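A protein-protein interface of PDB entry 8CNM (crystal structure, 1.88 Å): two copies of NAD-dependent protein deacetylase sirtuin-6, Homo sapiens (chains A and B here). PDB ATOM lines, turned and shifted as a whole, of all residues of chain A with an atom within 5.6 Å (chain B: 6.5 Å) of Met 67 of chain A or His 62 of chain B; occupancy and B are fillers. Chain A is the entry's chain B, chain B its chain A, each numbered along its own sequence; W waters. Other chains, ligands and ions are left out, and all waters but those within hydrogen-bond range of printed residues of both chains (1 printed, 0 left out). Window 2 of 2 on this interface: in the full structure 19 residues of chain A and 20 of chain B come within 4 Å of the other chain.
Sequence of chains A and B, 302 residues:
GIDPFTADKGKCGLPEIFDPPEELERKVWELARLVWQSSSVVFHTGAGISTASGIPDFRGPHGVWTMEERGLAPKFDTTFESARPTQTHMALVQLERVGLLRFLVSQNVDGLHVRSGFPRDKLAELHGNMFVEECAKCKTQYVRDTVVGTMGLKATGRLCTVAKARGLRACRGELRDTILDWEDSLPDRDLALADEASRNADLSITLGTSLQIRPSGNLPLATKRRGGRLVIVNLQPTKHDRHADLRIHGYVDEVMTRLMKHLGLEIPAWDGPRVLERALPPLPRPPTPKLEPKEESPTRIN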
ATOM      1  N   PHE A  58       8.590  -9.172  12.074  1.00  0.00           N
ATOM      2  CA  PHE A  58       7.683  -8.028  11.830  1.00  0.00           C
ATOM      3  C   PHE A  58       6.316  -8.232  12.501  1.00  0.00           C
ATOM      4  O   PHE A  58       5.828  -7.260  13.066  1.00  0.00           O
ATOM      5  CB  PHE A  58       7.533  -7.885  10.311  1.00  0.00           C
ATOM      6  CG  PHE A  58       8.762  -7.405   9.586  1.00  0.00           C
ATOM      7  CD1 PHE A  58       9.053  -6.054   9.505  1.00  0.00           C
ATOM      8  CD2 PHE A  58       9.629  -8.301   8.985  1.00  0.00           C
ATOM      9  CE1 PHE A  58      10.186  -5.610   8.845  1.00  0.00           C
ATOM     10  CE2 PHE A  58      10.764  -7.856   8.326  1.00  0.00           C
ATOM     11  CZ  PHE A  58      11.038  -6.512   8.255  1.00  0.00           C
ATOM     12  N   PRO A  61       5.050 -11.959  18.245  1.00  0.00           N
ATOM     13  CA  PRO A  61       4.652 -11.285  19.481  1.00  0.00           C
ATOM     14  C   PRO A  61       5.419  -9.971  19.699  1.00  0.00           C
ATOM     15  O   PRO A  61       4.780  -9.006  20.102  1.00  0.00           O
ATOM     16  CB  PRO A  61       4.945 -12.338  20.557  1.00  0.00           C
ATOM     17  CG  PRO A  61       4.738 -13.640  19.831  1.00  0.00           C
ATOM     18  CD  PRO A  61       5.262 -13.396  18.426  1.00  0.00           C
ATOM     19  N   HIS A  62       6.727  -9.941  19.395  1.00  0.00           N
ATOM     20  CA  HIS A  62       7.614  -8.755  19.555  1.00  0.00           C
ATOM     21  C   HIS A  62       8.118  -8.281  18.188  1.00  0.00           C
ATOM     22  O   HIS A  62       9.115  -7.531  18.131  1.00  0.00           O
ATOM     23  CB  HIS A  62       8.755  -9.023  20.550  1.00  0.00           C
ATOM     24  CG  HIS A  62       8.300  -9.196  21.965  1.00  0.00           C
ATOM     25  ND1 HIS A  62       9.187  -9.231  23.020  1.00  0.00           N
ATOM     26  CD2 HIS A  62       7.066  -9.353  22.507  1.00  0.00           C
ATOM     27  CE1 HIS A  62       8.533  -9.430  24.143  1.00  0.00           C
ATOM     28  NE2 HIS A  62       7.221  -9.501  23.861  1.00  0.00           N
ATOM     29  N   GLY A  63       7.384  -8.599  17.123  1.00  0.00           N
ATOM     30  CA  GLY A  63       7.714  -8.124  15.768  1.00  0.00           C
ATOM     31  C   GLY A  63       7.726  -6.609  15.639  1.00  0.00           C
ATOM     32  O   GLY A  63       7.042  -5.927  16.440  1.00  0.00           O
ATOM     33  N   VAL A  64       8.452  -6.097  14.642  1.00  0.00           N
ATOM     34  CA  VAL A  64       8.595  -4.644  14.320  1.00  0.00           C
ATOM     35  C   VAL A  64       7.188  -4.026  14.222  1.00  0.00           C
ATOM     36  O   VAL A  64       6.918  -3.094  14.987  1.00  0.00           O
ATOM     37  CB  VAL A  64       9.405  -4.414  13.028  1.00  0.00           C
ATOM     38  CG1 VAL A  64       9.403  -2.953  12.598  1.00  0.00           C
ATOM     39  CG2 VAL A  64      10.844  -4.904  13.143  1.00  0.00           C
ATOM     40  N   TRP A  65       6.322  -4.545  13.338  1.00  0.00           N
ATOM     41  CA  TRP A  65       4.956  -3.989  13.103  1.00  0.00           C
ATOM     42  C   TRP A  65       4.055  -4.245  14.323  1.00  0.00           C
ATOM     43  O   TRP A  65       3.282  -3.349  14.666  1.00  0.00           O
ATOM     44  CB  TRP A  65       4.302  -4.538  11.828  1.00  0.00           C
ATOM     45  CG  TRP A  65       5.085  -4.436  10.551  1.00  0.00           C
ATOM     46  CD1 TRP A  65       5.029  -5.329   9.523  1.00  0.00           C
ATOM     47  CD2 TRP A  65       5.966  -3.381  10.108  1.00  0.00           C
ATOM     48  NE1 TRP A  65       5.826  -4.925   8.487  1.00  0.00           N
ATOM     49  CE2 TRP A  65       6.409  -3.731   8.813  1.00  0.00           C
ATOM     50  CE3 TRP A  65       6.438  -2.191  10.674  1.00  0.00           C
ATOM     51  CZ2 TRP A  65       7.321  -2.952   8.097  1.00  0.00           C
ATOM     52  CZ3 TRP A  65       7.322  -1.411   9.962  1.00  0.00           C
ATOM     53  CH2 TRP A  65       7.763  -1.789   8.690  1.00  0.00           C
ATOM     54  N   THR A  66       4.139  -5.420  14.956  1.00  0.00           N
ATOM     55  CA  THR A  66       3.383  -5.757  16.196  1.00  0.00           C
ATOM     56  C   THR A  66       3.690  -4.715  17.280  1.00  0.00           C
ATOM     57  O   THR A  66       2.720  -4.161  17.866  1.00  0.00           O
ATOM     58  CB  THR A  66       3.727  -7.145  16.743  1.00  0.00           C
ATOM     59  OG1 THR A  66       3.630  -8.068  15.661  1.00  0.00           O
ATOM     60  CG2 THR A  66       2.817  -7.572  17.877  1.00  0.00           C
ATOM     61  N   MET A  67       4.977  -4.450  17.521  1.00  0.00           N
ATOM     62  CA  MET A  67       5.449  -3.500  18.562  1.00  0.00           C
ATOM     63  C   MET A  67       5.019  -2.071  18.188  1.00  0.00           C
ATOM     64  O   MET A  67       4.485  -1.370  19.066  1.00  0.00           O
ATOM     65  CB  MET A  67       6.969  -3.567  18.741  1.00  0.00           C
ATOM     66  CG  MET A  67       7.455  -4.850  19.417  1.00  0.00           C
ATOM     67  SD  MET A  67       6.509  -5.341  20.874  1.00  0.00           S
ATOM     68  CE  MET A  67       7.735  -5.169  22.167  1.00  0.00           C
ATOM     69  N   GLU A  68       5.182  -1.671  16.926  1.00  0.00           N
ATOM     70  CA  GLU A  68       4.679  -0.373  16.397  1.00  0.00           C
ATOM     71  C   GLU A  68       3.198  -0.179  16.787  1.00  0.00           C
ATOM     72  O   GLU A  68       2.874   0.891  17.348  1.00  0.00           O
ATOM     73  CB  GLU A  68       4.871  -0.324  14.880  1.00  0.00           C
ATOM     74  CG  GLU A  68       4.392   0.969  14.249  1.00  0.00           C
ATOM     75  CD  GLU A  68       4.546   1.035  12.738  1.00  0.00           C
ATOM     76  OE1 GLU A  68       3.895   0.227  12.036  1.00  0.00           O
ATOM     77  OE2 GLU A  68       5.321   1.888  12.267  1.00  0.00           O
ATOM     78  N   GLU A  69       2.334  -1.168  16.507  1.00  0.00           N
ATOM     79  CA  GLU A  69       0.867  -1.116  16.777  1.00  0.00           C
ATOM     80  C   GLU A  69       0.593  -0.887  18.266  1.00  0.00           C
ATOM     81  O   GLU A  69      -0.435  -0.273  18.575  1.00  0.00           O
ATOM     82  CB  GLU A  69       0.151  -2.420  16.426  1.00  0.00           C
ATOM     83  CG  GLU A  69      -0.143  -2.628  14.955  1.00  0.00           C
ATOM     84  CD  GLU A  69      -0.873  -3.938  14.693  1.00  0.00           C
ATOM     85  OE1 GLU A  69      -0.961  -4.766  15.633  1.00  0.00           O
ATOM     86  OE2 GLU A  69      -1.353  -4.137  13.562  1.00  0.00           O
ATOM     87  N   ARG A  70       1.447  -1.401  19.156  1.00  0.00           N
ATOM     88  CA  ARG A  70       1.227  -1.330  20.625  1.00  0.00           C
ATOM     89  C   ARG A  70       2.014  -0.164  21.207  1.00  0.00           C
ATOM     90  O   ARG A  70       2.114  -0.101  22.441  1.00  0.00           O
ATOM     91  CB  ARG A  70       1.599  -2.662  21.276  1.00  0.00           C
ATOM     92  CG  ARG A  70       0.733  -3.779  20.727  1.00  0.00           C
ATOM     93  CD  ARG A  70       1.021  -5.193  21.139  1.00  0.00           C
ATOM     94  NE  ARG A  70       0.292  -6.056  20.216  1.00  0.00           N
ATOM     95  CZ  ARG A  70      -0.754  -6.828  20.518  1.00  0.00           C
ATOM     96  NH1 ARG A  70      -1.384  -7.506  19.583  1.00  0.00           N
ATOM     97  NH2 ARG A  70      -1.185  -6.960  21.751  1.00  0.00           N
ATOM     98  N   GLY A  71       2.540   0.720  20.352  1.00  0.00           N
ATOM     99  CA  GLY A  71       3.301   1.909  20.772  1.00  0.00           C
ATOM    100  C   GLY A  71       4.602   1.542  21.463  1.00  0.00           C
ATOM    101  O   GLY A  71       5.057   2.325  22.300  1.00  0.00           O
ATOM    102  N   LEU A  72       5.192   0.394  21.124  1.00  0.00           N
ATOM    103  CA  LEU A  72       6.492  -0.068  21.678  1.00  0.00           C
ATOM    104  C   LEU A  72       7.495  -0.133  20.528  1.00  0.00           C
ATOM    105  O   LEU A  72       7.075   0.059  19.371  1.00  0.00           O
ATOM    106  CB  LEU A  72       6.276  -1.430  22.340  1.00  0.00           C
ATOM    107  CG  LEU A  72       5.297  -1.415  23.516  1.00  0.00           C
ATOM    108  CD1 LEU A  72       4.716  -2.799  23.773  1.00  0.00           C
ATOM    109  CD2 LEU A  72       5.968  -0.872  24.770  1.00  0.00           C
ATOM    110  N   ALA A  73       8.780  -0.321  20.822  1.00  0.00           N
ATOM    111  CA  ALA A  73       9.829  -0.440  19.783  1.00  0.00           C
ATOM    112  C   ALA A  73      10.272  -1.895  19.704  1.00  0.00           C
ATOM    113  O   ALA A  73      10.316  -2.589  20.718  1.00  0.00           O
ATOM    114  CB  ALA A  73      10.987   0.488  20.058  1.00  0.00           C
ATOM    115  N   PRO A  74      10.622  -2.399  18.501  1.00  0.00           N
ATOM    116  CA  PRO A  74      11.280  -3.700  18.385  1.00  0.00           C
ATOM    117  C   PRO A  74      12.690  -3.610  18.974  1.00  0.00           C
ATOM    118  O   PRO A  74      13.237  -2.512  19.059  1.00  0.00           O
ATOM    119  CB  PRO A  74      11.334  -3.936  16.873  1.00  0.00           C
ATOM    120  CG  PRO A  74      11.426  -2.537  16.317  1.00  0.00           C
ATOM    121  CD  PRO A  74      10.491  -1.731  17.196  1.00  0.00           C
ATOM    122  N   LYS A  75      13.256  -4.759  19.348  1.00  0.00           N
ATOM    123  CA  LYS A  75      14.568  -4.823  20.029  1.00  0.00           C
ATOM    124  C   LYS A  75      15.511  -5.692  19.185  1.00  0.00           C
ATOM    125  O   LYS A  75      15.198  -6.882  18.938  1.00  0.00           O
ATOM    126  CB  LYS A  75      14.326  -5.283  21.470  1.00  0.00           C
ATOM    127  CG  LYS A  75      15.555  -5.625  22.286  1.00  0.00           C
ATOM    128  CD  LYS A  75      16.623  -4.569  22.335  1.00  0.00           C
ATOM    129  CE  LYS A  75      17.817  -5.056  23.128  1.00  0.00           C
ATOM    130  NZ  LYS A  75      19.113  -4.612  22.558  1.00  0.00           N
ATOM    131  N   GLY B  13      14.964  -1.765  32.577  1.00  0.00           N
ATOM    132  CA  GLY B  13      14.581  -0.986  31.390  1.00  0.00           C
ATOM    133  C   GLY B  13      15.322   0.336  31.276  1.00  0.00           C
ATOM    134  O   GLY B  13      14.779   1.263  30.656  1.00  0.00           O
ATOM    135  N   PRO B  56      16.197 -13.997  26.143  1.00  0.00           N
ATOM    136  CA  PRO B  56      16.053 -12.631  26.595  1.00  0.00           C
ATOM    137  C   PRO B  56      16.823 -12.456  27.917  1.00  0.00           C
ATOM    138  O   PRO B  56      16.921 -13.436  28.648  1.00  0.00           O
ATOM    139  CB  PRO B  56      14.552 -12.461  26.767  1.00  0.00           C
ATOM    140  CG  PRO B  56      14.033 -13.844  27.063  1.00  0.00           C
ATOM    141  CD  PRO B  56      14.943 -14.767  26.268  1.00  0.00           C
ATOM    142  N   ASP B  57      17.386 -11.273  28.132  1.00  0.00           N
ATOM    143  CA  ASP B  57      18.033 -10.906  29.432  1.00  0.00           C
ATOM    144  C   ASP B  57      16.942 -10.614  30.474  1.00  0.00           C
ATOM    145  O   ASP B  57      15.743 -10.865  30.234  1.00  0.00           O
ATOM    146  CB  ASP B  57      19.049  -9.772  29.254  1.00  0.00           C
ATOM    147  CG  ASP B  57      18.521  -8.399  28.833  1.00  0.00           C
ATOM    148  OD1 ASP B  57      17.288  -8.199  28.854  1.00  0.00           O
ATOM    149  OD2 ASP B  57      19.335  -7.523  28.457  1.00  0.00           O
ATOM    150  N   PHE B  58      17.356 -10.129  31.639  1.00  0.00           N
ATOM    151  CA  PHE B  58      16.462  -9.815  32.778  1.00  0.00           C
ATOM    152  C   PHE B  58      16.036  -8.323  32.812  1.00  0.00           C
ATOM    153  O   PHE B  58      14.858  -8.086  33.039  1.00  0.00           O
ATOM    154  CB  PHE B  58      17.151 -10.316  34.058  1.00  0.00           C
ATOM    155  CG  PHE B  58      17.192 -11.820  34.125  1.00  0.00           C
ATOM    156  CD1 PHE B  58      16.077 -12.537  34.524  1.00  0.00           C
ATOM    157  CD2 PHE B  58      18.320 -12.525  33.714  1.00  0.00           C
ATOM    158  CE1 PHE B  58      16.115 -13.923  34.599  1.00  0.00           C
ATOM    159  CE2 PHE B  58      18.348 -13.906  33.755  1.00  0.00           C
ATOM    160  CZ  PHE B  58      17.239 -14.608  34.193  1.00  0.00           C
ATOM    161  N   ARG B  59      16.931  -7.351  32.578  1.00  0.00           N
ATOM    162  CA  ARG B  59      16.700  -5.931  32.904  1.00  0.00           C
ATOM    163  C   ARG B  59      16.953  -5.052  31.689  1.00  0.00           C
ATOM    164  O   ARG B  59      16.940  -3.842  31.853  1.00  0.00           O
ATOM    165  CB  ARG B  59      17.569  -5.529  34.102  1.00  0.00           C
ATOM    166  CG  ARG B  59      17.316  -6.458  35.281  1.00  0.00           C
ATOM    167  CD  ARG B  59      18.132  -6.051  36.509  1.00  0.00           C
ATOM    168  NE  ARG B  59      17.837  -6.956  37.590  1.00  0.00           N
ATOM    169  CZ  ARG B  59      18.347  -8.184  37.755  1.00  0.00           C
ATOM    170  NH1 ARG B  59      19.243  -8.683  36.912  1.00  0.00           N
ATOM    171  NH2 ARG B  59      17.975  -8.895  38.804  1.00  0.00           N
ATOM    172  N   GLY B  60      17.071  -5.656  30.502  1.00  0.00           N
ATOM    173  CA  GLY B  60      17.153  -4.915  29.226  1.00  0.00           C
ATOM    174  C   GLY B  60      15.790  -4.401  28.762  1.00  0.00           C
ATOM    175  O   GLY B  60      14.740  -4.683  29.335  1.00  0.00           O
ATOM    176  N   PRO B  61      15.731  -3.621  27.664  1.00  0.00           N
ATOM    177  CA  PRO B  61      14.468  -2.996  27.271  1.00  0.00           C
ATOM    178  C   PRO B  61      13.352  -4.058  27.216  1.00  0.00           C
ATOM    179  O   PRO B  61      12.235  -3.786  27.701  1.00  0.00           O
ATOM    180  CB  PRO B  61      14.795  -2.353  25.914  1.00  0.00           C
ATOM    181  CG  PRO B  61      16.295  -2.128  25.939  1.00  0.00           C
ATOM    182  CD  PRO B  61      16.856  -3.234  26.816  1.00  0.00           C
ATOM    183  N   HIS B  62      13.653  -5.251  26.700  1.00  0.00           N
ATOM    184  CA  HIS B  62      12.718  -6.407  26.636  1.00  0.00           C
ATOM    185  C   HIS B  62      13.138  -7.529  27.601  1.00  0.00           C
ATOM    186  O   HIS B  62      12.715  -8.686  27.419  1.00  0.00           O
ATOM    187  CB  HIS B  62      12.534  -6.876  25.182  1.00  0.00           C
ATOM    188  CG  HIS B  62      11.949  -5.829  24.284  1.00  0.00           C
ATOM    189  ND1 HIS B  62      11.525  -6.132  22.995  1.00  0.00           N
ATOM    190  CD2 HIS B  62      11.723  -4.503  24.440  1.00  0.00           C
ATOM    191  CE1 HIS B  62      11.075  -5.048  22.404  1.00  0.00           C
ATOM    192  NE2 HIS B  62      11.191  -4.023  23.254  1.00  0.00           N
ATOM    193  N   GLY B  63      13.798  -7.184  28.705  1.00  0.00           N
ATOM    194  CA  GLY B  63      14.141  -8.174  29.742  1.00  0.00           C
ATOM    195  C   GLY B  63      12.930  -8.815  30.407  1.00  0.00           C
ATOM    196  O   GLY B  63      11.842  -8.192  30.417  1.00  0.00           O
ATOM    197  N   VAL B  64      13.129 -10.006  30.987  1.00  0.00           N
ATOM    198  CA  VAL B  64      12.118 -10.805  31.746  1.00  0.00           C
ATOM    199  C   VAL B  64      11.489  -9.920  32.836  1.00  0.00           C
ATOM    200  O   VAL B  64      10.245  -9.775  32.823  1.00  0.00           O
ATOM    201  CB  VAL B  64      12.757 -12.076  32.349  1.00  0.00           C
ATOM    202  CG1 VAL B  64      11.827 -12.769  33.323  1.00  0.00           C
ATOM    203  CG2 VAL B  64      13.215 -13.058  31.280  1.00  0.00           C
ATOM    204  N   TRP B  65      12.297  -9.342  33.742  1.00  0.00           N
ATOM    205  CA  TRP B  65      11.790  -8.453  34.826  1.00  0.00           C
ATOM    206  C   TRP B  65      11.250  -7.128  34.265  1.00  0.00           C
ATOM    207  O   TRP B  65      10.223  -6.664  34.792  1.00  0.00           O
ATOM    208  CB  TRP B  65      12.849  -8.201  35.896  1.00  0.00           C
ATOM    209  CG  TRP B  65      13.540  -9.415  36.439  1.00  0.00           C
ATOM    210  CD1 TRP B  65      14.831  -9.452  36.878  1.00  0.00           C
ATOM    211  CD2 TRP B  65      12.987 -10.718  36.715  1.00  0.00           C
ATOM    212  NE1 TRP B  65      15.135 -10.692  37.368  1.00  0.00           N
ATOM    213  CE2 TRP B  65      14.024 -11.488  37.291  1.00  0.00           C
ATOM    214  CE3 TRP B  65      11.731 -11.317  36.539  1.00  0.00           C
ATOM    215  CZ2 TRP B  65      13.855 -12.824  37.644  1.00  0.00           C
ATOM    216  CZ3 TRP B  65      11.557 -12.636  36.897  1.00  0.00           C
ATOM    217  CH2 TRP B  65      12.610 -13.380  37.437  1.00  0.00           C
ATOM    218  N   THR B  66      11.904  -6.526  33.258  1.00  0.00           N
ATOM    219  CA  THR B  66      11.454  -5.267  32.602  1.00  0.00           C
ATOM    220  C   THR B  66      10.036  -5.431  32.050  1.00  0.00           C
ATOM    221  O   THR B  66       9.166  -4.548  32.341  1.00  0.00           O
ATOM    222  CB  THR B  66      12.360  -4.843  31.443  1.00  0.00           C
ATOM    223  OG1 THR B  66      13.694  -4.821  31.939  1.00  0.00           O
ATOM    224  CG2 THR B  66      11.954  -3.507  30.863  1.00  0.00           C
ATOM    225  N   MET B  67       9.842  -6.457  31.238  1.00  0.00           N
ATOM    226  CA  MET B  67       8.539  -6.824  30.634  1.00  0.00           C
ATOM    227  C   MET B  67       7.520  -7.125  31.749  1.00  0.00           C
ATOM    228  O   MET B  67       6.438  -6.529  31.726  1.00  0.00           O
ATOM    229  CB  MET B  67       8.700  -8.005  29.681  1.00  0.00           C
ATOM    230  CG  MET B  67       9.454  -7.655  28.400  1.00  0.00           C
ATOM    231  SD  MET B  67       8.882  -6.113  27.606  1.00  0.00           S
ATOM    232  CE  MET B  67       8.145  -6.760  26.110  1.00  0.00           C
ATOM    233  N   LEU B  72       3.941  -7.019  30.442  1.00  0.00           N
ATOM    234  CA  LEU B  72       4.142  -7.743  29.157  1.00  0.00           C
ATOM    235  C   LEU B  72       4.923  -9.023  29.458  1.00  0.00           C
ATOM    236  O   LEU B  72       5.228  -9.266  30.639  1.00  0.00           O
ATOM    237  CB  LEU B  72       4.863  -6.817  28.178  1.00  0.00           C
ATOM    238  CG  LEU B  72       4.131  -5.508  27.886  1.00  0.00           C
ATOM    239  CD1 LEU B  72       5.084  -4.410  27.450  1.00  0.00           C
ATOM    240  CD2 LEU B  72       3.047  -5.714  26.848  1.00  0.00           C
ATOM    241  N   ALA B  73       5.204  -9.831  28.442  1.00  0.00           N
ATOM    242  CA  ALA B  73       5.900 -11.128  28.604  1.00  0.00           C
ATOM    243  C   ALA B  73       7.206 -11.047  27.827  1.00  0.00           C
ATOM    244  O   ALA B  73       7.286 -10.373  26.792  1.00  0.00           O
ATOM    245  CB  ALA B  73       5.005 -12.264  28.178  1.00  0.00           C
ATOM    246  N   PRO B  74       8.308 -11.625  28.343  1.00  0.00           N
ATOM    247  CA  PRO B  74       9.533 -11.692  27.560  1.00  0.00           C
ATOM    248  C   PRO B  74       9.260 -12.650  26.393  1.00  0.00           C
ATOM    249  O   PRO B  74       8.315 -13.417  26.485  1.00  0.00           O
ATOM    250  CB  PRO B  74      10.547 -12.282  28.541  1.00  0.00           C
ATOM    251  CG  PRO B  74       9.675 -13.160  29.408  1.00  0.00           C
ATOM    252  CD  PRO B  74       8.434 -12.319  29.635  1.00  0.00           C
ATOM    253  N   LYS B  75      10.115 -12.623  25.374  1.00  0.00           N
ATOM    254  CA  LYS B  75       9.966 -13.484  24.179  1.00  0.00           C
ATOM    255  C   LYS B  75      11.277 -14.252  23.962  1.00  0.00           C
ATOM    256  O   LYS B  75      12.367 -13.627  23.901  1.00  0.00           O
ATOM    257  CB  LYS B  75       9.437 -12.604  23.040  1.00  0.00           C
ATOM    258  CG  LYS B  75       9.503 -13.171  21.642  1.00  0.00           C
ATOM    259  CD  LYS B  75       8.667 -14.376  21.377  1.00  0.00           C
ATOM    260  CE  LYS B  75       8.901 -14.876  19.963  1.00  0.00           C
ATOM    261  NZ  LYS B  75       8.871 -16.356  19.882  1.00  0.00           N
HETATM  262  O   HOH W   1      11.355  -6.951  19.635  1.00  0.00           O
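Printed residues of chain B within 4 Å of Met 67 of chain A: His 62.
His 62 of chain B touches just these residues of chain A: His 62, Met 67, Ala 73 and Lys 75.
Of the printed residues of chain B, His 62 of chain A touches His 62 (3.9 Å), Met 67 (3.3 Å), Ala 73 (3.1 Å), Pro 74 (3.99 Å) and Lys 75 (3.4 Å).
Of the printed residues of chain A, Met 67 of chain B touches His 62 (3.3 Å).
Printed residues of chain A within 4 Å of Lys 75 of chain B: His 62.
Of the printed residues of chain B, Lys 75 of chain A touches His 62 (3.3 Å).
Printed residues of chain A within 4 Å of Ala 73 of chain B: His 62 (3.1 Å).
Val 64 of chain A touches none of the printed residues of chain B.
The nearest residue of chain B that does not touch Met 67 of chain A is Met 67 of chain B (4.3 Å).
The nearest residue of chain A that does not touch His 62 of chain B is Pro 74 of chain A (4.1 Å).
O of Met 67 of chain B is in hydrogen-bond range of N of Leu 72 of chain B (2.9 Å).
O of Met 67 of chain A lies within hydrogen-bond range of N of Leu 72 of chain A (2.8 Å).
His 62 of chain B touches its own counterpart, His 62 of chain A.
His 62 of chain A touches Met 67 of chain B, and with the chains exchanged Met 67 of chain A touches His 62 of chain B.
His 62 of chain A touches Pro 74 of chain B, but with the chains exchanged Pro 74 of chain A does not touch His 62 of chain B (4.1 Å).
His 62 of chain A touches Lys 75 of chain B, and with the chains exchanged Lys 75 of chain A touches His 62 of chain B.
12 positions are printed for both chains.
Among the printed residues, pairs that only touch across the chains: His 62 of chain A with His 62 of chain B (3.9 Å), His 62 of chain A with Met 67 of chain B (3.3 Å), His 62 of chain A with Pro 74 of chain B (3.99 Å), His 62 of chain A with Lys 75 of chain B (3.4 Å), Met 67 of chain A with His 62 of chain B (3.4 Å) and Lys 75 of chain A with His 62 of chain B (3.3 Å).
A ring nitrogen (NE2) of His 62 of chain B sits at hydrogen-bond distance from the backbone carbonyl oxygen (O) of Ala 73 of chain A, at 3.0 Å.
A ring nitrogen (NE2) of His 62 of chain A lies within hydrogen-bond range of the backbone carbonyl oxygen of Ala 73 of chain B (3.1 Å).
Water W1 lies within hydrogen-bond range of the backbone carbonyl oxygen (O) of His 62 of chain A (2.8 Å), the backbone NH (N) of Lys 75 of chain A (2.9 Å) and a ring nitrogen (ND1) of His 62 of chain B (3.5 Å).
Of the 16 printed residues of chain A, 4 touch a printed residue of chain B.
Hydrophobic or aromatic side chains of chain A that line the printed part of chain B: His 62 and Met 67.
Printed residues of chain B that touch a printed residue of chain A: His 62, Met 67, Ala 73, Pro 74 and Lys 75.
Among the printed residues, 8 pairs touch across the chains.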
